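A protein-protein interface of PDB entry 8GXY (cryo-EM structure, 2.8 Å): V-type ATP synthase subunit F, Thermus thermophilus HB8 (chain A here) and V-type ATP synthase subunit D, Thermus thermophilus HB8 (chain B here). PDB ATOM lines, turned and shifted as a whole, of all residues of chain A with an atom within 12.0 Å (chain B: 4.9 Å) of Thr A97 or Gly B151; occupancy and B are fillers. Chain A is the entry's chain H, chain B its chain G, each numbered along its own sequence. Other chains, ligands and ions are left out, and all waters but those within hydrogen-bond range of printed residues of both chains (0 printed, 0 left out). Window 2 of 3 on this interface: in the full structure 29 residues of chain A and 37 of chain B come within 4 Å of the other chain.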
ATOM      1  N   ASP A  54     -30.890 -29.294 -21.046  1.00  0.00           N
ATOM      2  CA  ASP A  54     -30.000 -28.245 -21.525  1.00  0.00           C
ATOM      3  C   ASP A  54     -30.774 -27.244 -22.372  1.00  0.00           C
ATOM      4  O   ASP A  54     -30.881 -27.421 -23.593  1.00  0.00           O
ATOM      5  CB  ASP A  54     -28.852 -28.849 -22.334  1.00  0.00           C
ATOM      6  CG  ASP A  54     -27.849 -29.579 -21.465  1.00  0.00           C
ATOM      7  OD1 ASP A  54     -28.180 -29.875 -20.298  1.00  0.00           O
ATOM      8  OD2 ASP A  54     -26.730 -29.854 -21.947  1.00  0.00           O
ATOM      9  N   GLU A  56     -30.003 -24.351 -23.475  1.00  0.00           N
ATOM     10  CA  GLU A  56     -29.171 -23.828 -24.550  1.00  0.00           C
ATOM     11  C   GLU A  56     -29.111 -24.808 -25.712  1.00  0.00           C
ATOM     12  O   GLU A  56     -29.234 -24.412 -26.875  1.00  0.00           O
ATOM     13  CB  GLU A  56     -27.767 -23.509 -24.031  1.00  0.00           C
ATOM     14  CG  GLU A  56     -27.093 -24.628 -23.243  1.00  0.00           C
ATOM     15  CD  GLU A  56     -27.351 -24.534 -21.751  1.00  0.00           C
ATOM     16  OE1 GLU A  56     -28.421 -24.020 -21.363  1.00  0.00           O
ATOM     17  OE2 GLU A  56     -26.484 -24.974 -20.968  1.00  0.00           O
ATOM     18  N   LEU A  71     -30.618 -18.445 -20.026  1.00  0.00           N
ATOM     19  CA  LEU A  71     -31.298 -19.699 -19.749  1.00  0.00           C
ATOM     20  C   LEU A  71     -30.663 -20.347 -18.531  1.00  0.00           C
ATOM     21  O   LEU A  71     -29.441 -20.295 -18.357  1.00  0.00           O
ATOM     22  CB  LEU A  71     -31.226 -20.650 -20.942  1.00  0.00           C
ATOM     23  CG  LEU A  71     -31.670 -20.085 -22.291  1.00  0.00           C
ATOM     24  CD1 LEU A  71     -31.477 -21.128 -23.377  1.00  0.00           C
ATOM     25  CD2 LEU A  71     -33.114 -19.625 -22.233  1.00  0.00           C
ATOM     26  N   GLU A  87     -23.117 -31.748  -7.144  1.00  0.00           N
ATOM     27  CA  GLU A  87     -21.755 -32.004  -7.596  1.00  0.00           C
ATOM     28  C   GLU A  87     -21.748 -32.583  -9.002  1.00  0.00           C
ATOM     29  O   GLU A  87     -20.884 -32.242  -9.819  1.00  0.00           O
ATOM     30  CB  GLU A  87     -21.052 -32.944  -6.618  1.00  0.00           C
ATOM     31  CG  GLU A  87     -19.644 -33.349  -7.043  1.00  0.00           C
ATOM     32  CD  GLU A  87     -19.617 -34.616  -7.882  1.00  0.00           C
ATOM     33  OE1 GLU A  87     -20.578 -35.410  -7.806  1.00  0.00           O
ATOM     34  OE2 GLU A  87     -18.631 -34.818  -8.620  1.00  0.00           O
ATOM     35  N   GLY A  88     -22.704 -33.458  -9.309  1.00  0.00           N
ATOM     36  CA  GLY A  88     -22.778 -34.007 -10.650  1.00  0.00           C
ATOM     37  C   GLY A  88     -23.076 -32.947 -11.690  1.00  0.00           C
ATOM     38  O   GLY A  88     -22.509 -32.960 -12.788  1.00  0.00           O
ATOM     39  N   TYR A  89     -23.970 -32.013 -11.364  1.00  0.00           N
ATOM     40  CA  TYR A  89     -24.287 -30.955 -12.312  1.00  0.00           C
ATOM     41  C   TYR A  89     -23.051 -30.132 -12.639  1.00  0.00           C
ATOM     42  O   TYR A  89     -22.789 -29.823 -13.807  1.00  0.00           O
ATOM     43  CB  TYR A  89     -25.384 -30.054 -11.752  1.00  0.00           C
ATOM     44  CG  TYR A  89     -25.547 -28.784 -12.546  1.00  0.00           C
ATOM     45  CD1 TYR A  89     -25.586 -28.816 -13.931  1.00  0.00           C
ATOM     46  CD2 TYR A  89     -25.627 -27.554 -11.917  1.00  0.00           C
ATOM     47  CE1 TYR A  89     -25.723 -27.664 -14.663  1.00  0.00           C
ATOM     48  CE2 TYR A  89     -25.762 -26.397 -12.642  1.00  0.00           C
ATOM     49  CZ  TYR A  89     -25.810 -26.456 -14.016  1.00  0.00           C
ATOM     50  OH  TYR A  89     -25.946 -25.298 -14.746  1.00  0.00           O
ATOM     51  N   MET A  90     -22.275 -29.766 -11.621  1.00  0.00           N
ATOM     52  CA  MET A  90     -21.090 -28.959 -11.875  1.00  0.00           C
ATOM     53  C   MET A  90     -20.010 -29.773 -12.569  1.00  0.00           C
ATOM     54  O   MET A  90     -19.219 -29.224 -13.338  1.00  0.00           O
ATOM     55  CB  MET A  90     -20.561 -28.362 -10.575  1.00  0.00           C
ATOM     56  CG  MET A  90     -21.197 -27.029 -10.204  1.00  0.00           C
ATOM     57  SD  MET A  90     -21.082 -25.741 -11.465  1.00  0.00           S
ATOM     58  CE  MET A  90     -19.472 -26.060 -12.186  1.00  0.00           C
ATOM     59  N   ARG A  91     -19.947 -31.078 -12.309  1.00  0.00           N
ATOM     60  CA  ARG A  91     -19.037 -31.919 -13.077  1.00  0.00           C
ATOM     61  C   ARG A  91     -19.391 -31.871 -14.557  1.00  0.00           C
ATOM     62  O   ARG A  91     -18.513 -31.703 -15.416  1.00  0.00           O
ATOM     63  CB  ARG A  91     -19.088 -33.353 -12.556  1.00  0.00           C
ATOM     64  CG  ARG A  91     -17.944 -34.231 -13.022  1.00  0.00           C
ATOM     65  CD  ARG A  91     -17.966 -35.583 -12.326  1.00  0.00           C
ATOM     66  NE  ARG A  91     -17.641 -35.475 -10.909  1.00  0.00           N
ATOM     67  CZ  ARG A  91     -16.413 -35.542 -10.409  1.00  0.00           C
ATOM     68  NH1 ARG A  91     -15.355 -35.708 -11.187  1.00  0.00           N
ATOM     69  NH2 ARG A  91     -16.242 -35.439  -9.094  1.00  0.00           N
ATOM     70  N   GLU A  92     -20.680 -31.982 -14.870  1.00  0.00           N
ATOM     71  CA  GLU A  92     -21.113 -31.893 -16.260  1.00  0.00           C
ATOM     72  C   GLU A  92     -20.800 -30.523 -16.843  1.00  0.00           C
ATOM     73  O   GLU A  92     -20.393 -30.413 -18.004  1.00  0.00           O
ATOM     74  CB  GLU A  92     -22.608 -32.188 -16.363  1.00  0.00           C
ATOM     75  CG  GLU A  92     -23.147 -32.158 -17.784  1.00  0.00           C
ATOM     76  CD  GLU A  92     -24.457 -32.908 -17.925  1.00  0.00           C
ATOM     77  OE1 GLU A  92     -25.238 -32.934 -16.951  1.00  0.00           O
ATOM     78  OE2 GLU A  92     -24.706 -33.472 -19.012  1.00  0.00           O
ATOM     79  N   LEU A  93     -20.982 -29.463 -16.053  1.00  0.00           N
ATOM     80  CA  LEU A  93     -20.737 -28.115 -16.560  1.00  0.00           C
ATOM     81  C   LEU A  93     -19.250 -27.867 -16.792  1.00  0.00           C
ATOM     82  O   LEU A  93     -18.870 -27.213 -17.767  1.00  0.00           O
ATOM     83  CB  LEU A  93     -21.312 -27.083 -15.593  1.00  0.00           C
ATOM     84  CG  LEU A  93     -21.584 -25.668 -16.117  1.00  0.00           C
ATOM     85  CD1 LEU A  93     -21.954 -25.643 -17.593  1.00  0.00           C
ATOM     86  CD2 LEU A  93     -22.681 -25.018 -15.292  1.00  0.00           C
ATOM     87  N   VAL A  94     -18.395 -28.377 -15.910  1.00  0.00           N
ATOM     88  CA  VAL A  94     -16.957 -28.278 -16.127  1.00  0.00           C
ATOM     89  C   VAL A  94     -16.561 -29.041 -17.382  1.00  0.00           C
ATOM     90  O   VAL A  94     -15.748 -28.566 -18.182  1.00  0.00           O
ATOM     91  CB  VAL A  94     -16.193 -28.780 -14.891  1.00  0.00           C
ATOM     92  CG1 VAL A  94     -14.714 -28.914 -15.201  1.00  0.00           C
ATOM     93  CG2 VAL A  94     -16.408 -27.837 -13.724  1.00  0.00           C
ATOM     94  N   ARG A  95     -17.127 -30.234 -17.577  1.00  0.00           N
ATOM     95  CA  ARG A  95     -16.865 -30.965 -18.813  1.00  0.00           C
ATOM     96  C   ARG A  95     -17.305 -30.152 -20.023  1.00  0.00           C
ATOM     97  O   ARG A  95     -16.611 -30.116 -21.045  1.00  0.00           O
ATOM     98  CB  ARG A  95     -17.578 -32.318 -18.784  1.00  0.00           C
ATOM     99  CG  ARG A  95     -17.516 -33.111 -20.091  1.00  0.00           C
ATOM    100  CD  ARG A  95     -18.661 -34.110 -20.178  1.00  0.00           C
ATOM    101  NE  ARG A  95     -18.599 -35.111 -19.118  1.00  0.00           N
ATOM    102  CZ  ARG A  95     -19.627 -35.848 -18.721  1.00  0.00           C
ATOM    103  NH1 ARG A  95     -20.822 -35.729 -19.278  1.00  0.00           N
ATOM    104  NH2 ARG A  95     -19.452 -36.729 -17.741  1.00  0.00           N
ATOM    105  N   LYS A  96     -18.461 -29.496 -19.927  1.00  0.00           N
ATOM    106  CA  LYS A  96     -18.957 -28.695 -21.040  1.00  0.00           C
ATOM    107  C   LYS A  96     -18.070 -27.488 -21.307  1.00  0.00           C
ATOM    108  O   LYS A  96     -17.940 -27.062 -22.459  1.00  0.00           O
ATOM    109  CB  LYS A  96     -20.387 -28.234 -20.756  1.00  0.00           C
ATOM    110  CG  LYS A  96     -21.443 -29.311 -20.949  1.00  0.00           C
ATOM    111  CD  LYS A  96     -22.000 -29.309 -22.365  1.00  0.00           C
ATOM    112  CE  LYS A  96     -22.998 -28.178 -22.576  1.00  0.00           C
ATOM    113  NZ  LYS A  96     -24.276 -28.415 -21.851  1.00  0.00           N
ATOM    114  N   THR A  97     -17.461 -26.926 -20.266  1.00  0.00           N
ATOM    115  CA  THR A  97     -16.727 -25.674 -20.399  1.00  0.00           C
ATOM    116  C   THR A  97     -15.270 -25.871 -20.795  1.00  0.00           C
ATOM    117  O   THR A  97     -14.774 -25.155 -21.671  1.00  0.00           O
ATOM    118  CB  THR A  97     -16.796 -24.885 -19.089  1.00  0.00           C
ATOM    119  OG1 THR A  97     -16.631 -25.775 -17.979  1.00  0.00           O
ATOM    120  CG2 THR A  97     -18.131 -24.173 -18.968  1.00  0.00           C
ATOM    121  N   ILE A  98     -14.565 -26.818 -20.182  1.00  0.00           N
ATOM    122  CA  ILE A  98     -13.151 -27.030 -20.470  1.00  0.00           C
ATOM    123  C   ILE A  98     -12.878 -28.342 -21.189  1.00  0.00           C
ATOM    124  O   ILE A  98     -11.790 -28.495 -21.765  1.00  0.00           O
ATOM    125  CB  ILE A  98     -12.291 -26.944 -19.189  1.00  0.00           C
ATOM    126  CG1 ILE A  98     -12.639 -28.065 -18.213  1.00  0.00           C
ATOM    127  CG2 ILE A  98     -12.482 -25.595 -18.522  1.00  0.00           C
ATOM    128  CD1 ILE A  98     -11.671 -28.179 -17.058  1.00  0.00           C
ATOM    129  N   GLY A  99     -13.808 -29.294 -21.180  1.00  0.00           N
ATOM    130  CA  GLY A  99     -13.648 -30.512 -21.949  1.00  0.00           C
ATOM    131  C   GLY A  99     -12.878 -31.614 -21.247  1.00  0.00           C
ATOM    132  O   GLY A  99     -13.050 -32.794 -21.566  1.00  0.00           O
ATOM    133  N   PHE A 100     -12.028 -31.248 -20.289  1.00  0.00           N
ATOM    134  CA  PHE A 100     -11.184 -32.245 -19.637  1.00  0.00           C
ATOM    135  C   PHE A 100     -12.012 -33.252 -18.852  1.00  0.00           C
ATOM    136  O   PHE A 100     -11.707 -34.449 -18.851  1.00  0.00           O
ATOM    137  CB  PHE A 100     -10.176 -31.556 -18.718  1.00  0.00           C
ATOM    138  CG  PHE A 100      -8.987 -30.977 -19.435  1.00  0.00           C
ATOM    139  CD1 PHE A 100      -8.897 -31.003 -20.819  1.00  0.00           C
ATOM    140  CD2 PHE A 100      -7.947 -30.418 -18.715  1.00  0.00           C
ATOM    141  CE1 PHE A 100      -7.797 -30.471 -21.465  1.00  0.00           C
ATOM    142  CE2 PHE A 100      -6.847 -29.888 -19.355  1.00  0.00           C
ATOM    143  CZ  PHE A 100      -6.772 -29.916 -20.732  1.00  0.00           C
ATOM    144  N   ASP A 101     -13.061 -32.791 -18.172  1.00  0.00           N
ATOM    145  CA  ASP A 101     -13.898 -33.657 -17.345  1.00  0.00           C
ATOM    146  C   ASP A 101     -13.057 -34.325 -16.253  1.00  0.00           C
ATOM    147  O   ASP A 101     -12.871 -35.542 -16.213  1.00  0.00           O
ATOM    148  CB  ASP A 101     -14.612 -34.707 -18.205  1.00  0.00           C
ATOM    149  CG  ASP A 101     -15.700 -35.440 -17.445  1.00  0.00           C
ATOM    150  OD1 ASP A 101     -15.950 -35.091 -16.272  1.00  0.00           O
ATOM    151  OD2 ASP A 101     -16.307 -36.366 -18.022  1.00  0.00           O
ATOM    152  N   ILE A 102     -12.539 -33.478 -15.371  1.00  0.00           N
ATOM    153  CA  ILE A 102     -11.627 -33.911 -14.320  1.00  0.00           C
ATOM    154  C   ILE A 102     -11.842 -33.029 -13.099  1.00  0.00           C
ATOM    155  O   ILE A 102     -11.873 -31.801 -13.208  1.00  0.00           O
ATOM    156  CB  ILE A 102     -10.163 -33.855 -14.804  1.00  0.00           C
ATOM    157  CG1 ILE A 102      -9.800 -35.152 -15.533  1.00  0.00           C
ATOM    158  CG2 ILE A 102      -9.214 -33.614 -13.646  1.00  0.00           C
ATOM    159  CD1 ILE A 102      -8.511 -35.077 -16.321  1.00  0.00           C
ATOM    160  N   LYS A 103     -11.981 -33.660 -11.936  1.00  0.00           N
ATOM    161  CA  LYS A 103     -12.165 -32.952 -10.676  1.00  0.00           C
ATOM    162  C   LYS A 103     -12.221 -33.976  -9.550  1.00  0.00           C
ATOM    163  O   LYS A 103     -12.476 -35.161  -9.779  1.00  0.00           O
ATOM    164  CB  LYS A 103     -13.442 -32.105 -10.689  1.00  0.00           C
ATOM    165  CG  LYS A 103     -13.794 -31.465  -9.355  1.00  0.00           C
ATOM    166  CD  LYS A 103     -14.991 -30.544  -9.476  1.00  0.00           C
ATOM    167  CE  LYS A 103     -15.246 -29.810  -8.177  1.00  0.00           C
ATOM    168  NZ  LYS A 103     -15.416 -30.743  -7.030  1.00  0.00           N
ATOM    169  N   PHE B  39     -11.277 -19.621 -13.083  1.00  0.00           N
ATOM    170  CA  PHE B  39     -12.367 -20.545 -13.364  1.00  0.00           C
ATOM    171  C   PHE B  39     -12.623 -21.470 -12.187  1.00  0.00           C
ATOM    172  O   PHE B  39     -13.778 -21.740 -11.837  1.00  0.00           O
ATOM    173  CB  PHE B  39     -12.036 -21.359 -14.610  1.00  0.00           C
ATOM    174  CG  PHE B  39     -13.111 -22.318 -15.018  1.00  0.00           C
ATOM    175  CD1 PHE B  39     -14.156 -21.906 -15.815  1.00  0.00           C
ATOM    176  CD2 PHE B  39     -13.064 -23.634 -14.621  1.00  0.00           C
ATOM    177  CE1 PHE B  39     -15.136 -22.789 -16.196  1.00  0.00           C
ATOM    178  CE2 PHE B  39     -14.038 -24.513 -15.001  1.00  0.00           C
ATOM    179  CZ  PHE B  39     -15.075 -24.090 -15.791  1.00  0.00           C
ATOM    180  N   LEU B 147     -19.032 -17.806 -15.425  1.00  0.00           N
ATOM    181  CA  LEU B 147     -18.296 -19.064 -15.494  1.00  0.00           C
ATOM    182  C   LEU B 147     -18.188 -19.548 -16.933  1.00  0.00           C
ATOM    183  O   LEU B 147     -17.106 -19.932 -17.397  1.00  0.00           O
ATOM    184  CB  LEU B 147     -18.983 -20.113 -14.624  1.00  0.00           C
ATOM    185  CG  LEU B 147     -18.315 -21.484 -14.559  1.00  0.00           C
ATOM    186  CD1 LEU B 147     -18.450 -22.067 -13.173  1.00  0.00           C
ATOM    187  CD2 LEU B 147     -18.918 -22.426 -15.581  1.00  0.00           C
ATOM    188  N   LYS B 148     -19.306 -19.538 -17.658  1.00  0.00           N
ATOM    189  CA  LYS B 148     -19.289 -19.995 -19.042  1.00  0.00           C
ATOM    190  C   LYS B 148     -18.396 -19.112 -19.898  1.00  0.00           C
ATOM    191  O   LYS B 148     -17.701 -19.601 -20.795  1.00  0.00           O
ATOM    192  CB  LYS B 148     -20.707 -20.024 -19.604  1.00  0.00           C
ATOM    193  CG  LYS B 148     -21.595 -21.083 -18.984  1.00  0.00           C
ATOM    194  CD  LYS B 148     -22.994 -21.027 -19.557  1.00  0.00           C
ATOM    195  CE  LYS B 148     -23.892 -22.082 -18.937  1.00  0.00           C
ATOM    196  NZ  LYS B 148     -25.275 -22.028 -19.486  1.00  0.00           N
ATOM    197  N   LYS B 149     -18.413 -17.803 -19.650  1.00  0.00           N
ATOM    198  CA  LYS B 149     -17.551 -16.908 -20.417  1.00  0.00           C
ATOM    199  C   LYS B 149     -16.076 -17.211 -20.173  1.00  0.00           C
ATOM    200  O   LYS B 149     -15.269 -17.233 -21.112  1.00  0.00           O
ATOM    201  CB  LYS B 149     -17.870 -15.458 -20.070  1.00  0.00           C
ATOM    202  CG  LYS B 149     -19.256 -15.013 -20.518  1.00  0.00           C
ATOM    203  CD  LYS B 149     -19.467 -15.161 -22.023  1.00  0.00           C
ATOM    204  CE  LYS B 149     -18.339 -14.554 -22.846  1.00  0.00           C
ATOM    205  NZ  LYS B 149     -17.851 -13.245 -22.332  1.00  0.00           N
ATOM    206  N   ILE B 150     -15.699 -17.445 -18.916  1.00  0.00           N
ATOM    207  CA  ILE B 150     -14.316 -17.813 -18.622  1.00  0.00           C
ATOM    208  C   ILE B 150     -13.958 -19.112 -19.329  1.00  0.00           C
ATOM    209  O   ILE B 150     -12.851 -19.266 -19.861  1.00  0.00           O
ATOM    210  CB  ILE B 150     -14.095 -17.926 -17.104  1.00  0.00           C
ATOM    211  CG1 ILE B 150     -14.231 -16.560 -16.433  1.00  0.00           C
ATOM    212  CG2 ILE B 150     -12.733 -18.519 -16.817  1.00  0.00           C
ATOM    213  CD1 ILE B 150     -12.994 -15.700 -16.526  1.00  0.00           C
ATOM    214  N   GLY B 151     -14.878 -20.074 -19.330  1.00  0.00           N
ATOM    215  CA  GLY B 151     -14.616 -21.327 -20.017  1.00  0.00           C
ATOM    216  C   GLY B 151     -14.393 -21.137 -21.503  1.00  0.00           C
ATOM    217  O   GLY B 151     -13.505 -21.755 -22.095  1.00  0.00           O
ATOM    218  N   GLU B 152     -15.200 -20.285 -22.130  1.00  0.00           N
ATOM    219  CA  GLU B 152     -15.023 -20.021 -23.552  1.00  0.00           C
ATOM    220  C   GLU B 152     -13.698 -19.331 -23.827  1.00  0.00           C
ATOM    221  O   GLU B 152     -13.047 -19.617 -24.839  1.00  0.00           O
ATOM    222  CB  GLU B 152     -16.181 -19.180 -24.077  1.00  0.00           C
ATOM    223  CG  GLU B 152     -17.486 -19.945 -24.179  1.00  0.00           C
ATOM    224  CD  GLU B 152     -18.603 -19.117 -24.778  1.00  0.00           C
ATOM    225  OE1 GLU B 152     -18.415 -17.892 -24.939  1.00  0.00           O
ATOM    226  OE2 GLU B 152     -19.667 -19.689 -25.091  1.00  0.00           O
ATOM    227  N   GLU B 153     -13.282 -18.422 -22.949  1.00  0.00           N
ATOM    228  CA  GLU B 153     -11.976 -17.794 -23.113  1.00  0.00           C
ATOM    229  C   GLU B 153     -10.852 -18.819 -22.992  1.00  0.00           C
ATOM    230  O   GLU B 153      -9.870 -18.766 -23.744  1.00  0.00           O
ATOM    231  CB  GLU B 153     -11.809 -16.681 -22.085  1.00  0.00           C
ATOM    232  CG  GLU B 153     -11.112 -15.451 -22.616  1.00  0.00           C
ATOM    233  CD  GLU B 153     -10.502 -14.619 -21.510  1.00  0.00           C
ATOM    234  OE1 GLU B 153     -11.008 -14.692 -20.370  1.00  0.00           O
ATOM    235  OE2 GLU B 153      -9.521 -13.894 -21.777  1.00  0.00           O
ATOM    236  N   ILE B 154     -10.978 -19.760 -22.055  1.00  0.00           N
ATOM    237  CA  ILE B 154      -9.979 -20.819 -21.936  1.00  0.00           C
ATOM    238  C   ILE B 154      -9.943 -21.655 -23.208  1.00  0.00           C
ATOM    239  O   ILE B 154      -8.870 -22.045 -23.682  1.00  0.00           O
ATOM    240  CB  ILE B 154     -10.257 -21.696 -20.703  1.00  0.00           C
ATOM    241  CG1 ILE B 154      -9.887 -20.955 -19.422  1.00  0.00           C
ATOM    242  CG2 ILE B 154      -9.473 -22.981 -20.791  1.00  0.00           C
ATOM    243  CD1 ILE B 154     -10.491 -21.555 -18.180  1.00  0.00           C
ATOM    244  N   LYS B 155     -11.112 -21.959 -23.768  1.00  0.00           N
ATOM    245  CA  LYS B 155     -11.152 -22.714 -25.016  1.00  0.00           C
ATOM    246  C   LYS B 155     -10.460 -21.955 -26.141  1.00  0.00           C
ATOM    247  O   LYS B 155      -9.705 -22.543 -26.924  1.00  0.00           O
ATOM    248  CB  LYS B 155     -12.599 -23.025 -25.395  1.00  0.00           C
ATOM    249  CG  LYS B 155     -12.938 -24.499 -25.378  1.00  0.00           C
ATOM    250  CD  LYS B 155     -14.398 -24.740 -25.041  1.00  0.00           C
ATOM    251  CE  LYS B 155     -14.631 -26.167 -24.573  1.00  0.00           C
ATOM    252  NZ  LYS B 155     -15.918 -26.312 -23.838  1.00  0.00           N
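The side-chain amino group (NZ) of Lys A96 lies within salt-bridge range of the side-chain carboxylate (OD2) of Asp A54, 2.8 Å away.
O of Val A94 is in hydrogen-bond range of OG1 of Thr A97 (2.9 Å).
O of Leu A93 lies within hydrogen-bond range of OG1 of Thr A97 (2.7 Å).
Among the printed residues, pairs that only touch across the chains: Thr A97 with Phe B39, Thr A97 with Gly B151, Thr A97 with Leu B147, Ile A98 with Lys B155 and Ile A98 with Phe B39.
OE2 of Glu A56 is in salt-bridge range of NZ of Lys B148, at 3.5 Å.
The side-chain amino group of Lys B155 sits at hydrogen-bond distance from the backbone carbonyl oxygen of Thr A97, 2.7 Å away.
The backbone carbonyl oxygen (O) of Lys A96 sits at hydrogen-bond distance from the side-chain amino group (NZ) of Lys B155, 2.6 Å away.
Of the 20 printed residues of chain A, 4 touch a printed residue of chain B.
Printed residues of chain A that touch a printed residue of chain B: Glu A56, Lys A96, Thr A97 and Ile A98.
Hydrophobic or aromatic side chains of chain A that line the printed part of chain B: Ile A98.
Among the printed residues, 8 pairs touch across the chains.
Among the printed residues, Asp or Glu carboxylates within 4 Å of a Lys or Arg side-chain nitrogen of the other chain: Glu A56 with Lys B148 (3.5 Å).
Of the printed residues of chain B, Glu A56 touches Lys B148.
Met A90 touches none of the printed residues of chain B.
Of the printed residues of chain B, Lys A96 touches Lys B155.
Thr A97 touches just these residues of chain B: Phe B39, Leu B147, Gly B151 and Lys B155.
Printed residues of chain B within 4 Å of Ile A98: Phe B39 (3.999 Å) and Lys B155 (3.9 Å).
Phe A100 touches none of the printed residues of chain B.
Printed residues of chain A within 4 Å of Phe B39: Thr A97 (3.2 Å) and Ile A98 (3.999 Å).
Leu B147 touches just one residue of chain A: Thr A97.
Of chain A, only Glu A56 comes within 4 Å of Lys B148.
No residue of chain A comes within 4 Å of Ile B150.
Of chain A, only Thr A97 comes within 4 Å of Gly B151.
No residue of chain A comes within 4 Å of Glu B152.
No residue of chain A comes within 4 Å of Ile B154.
Of chain A, only Lys A96, Thr A97 and Ile A98 come within 4 Å of Lys B155.
The nearest residue of chain A that does not touch Gly B151 is Ile A98 (5.0 Å).
The nearest printed residue of chain B that does not touch Glu A56 is Glu B152 (9.0 Å).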
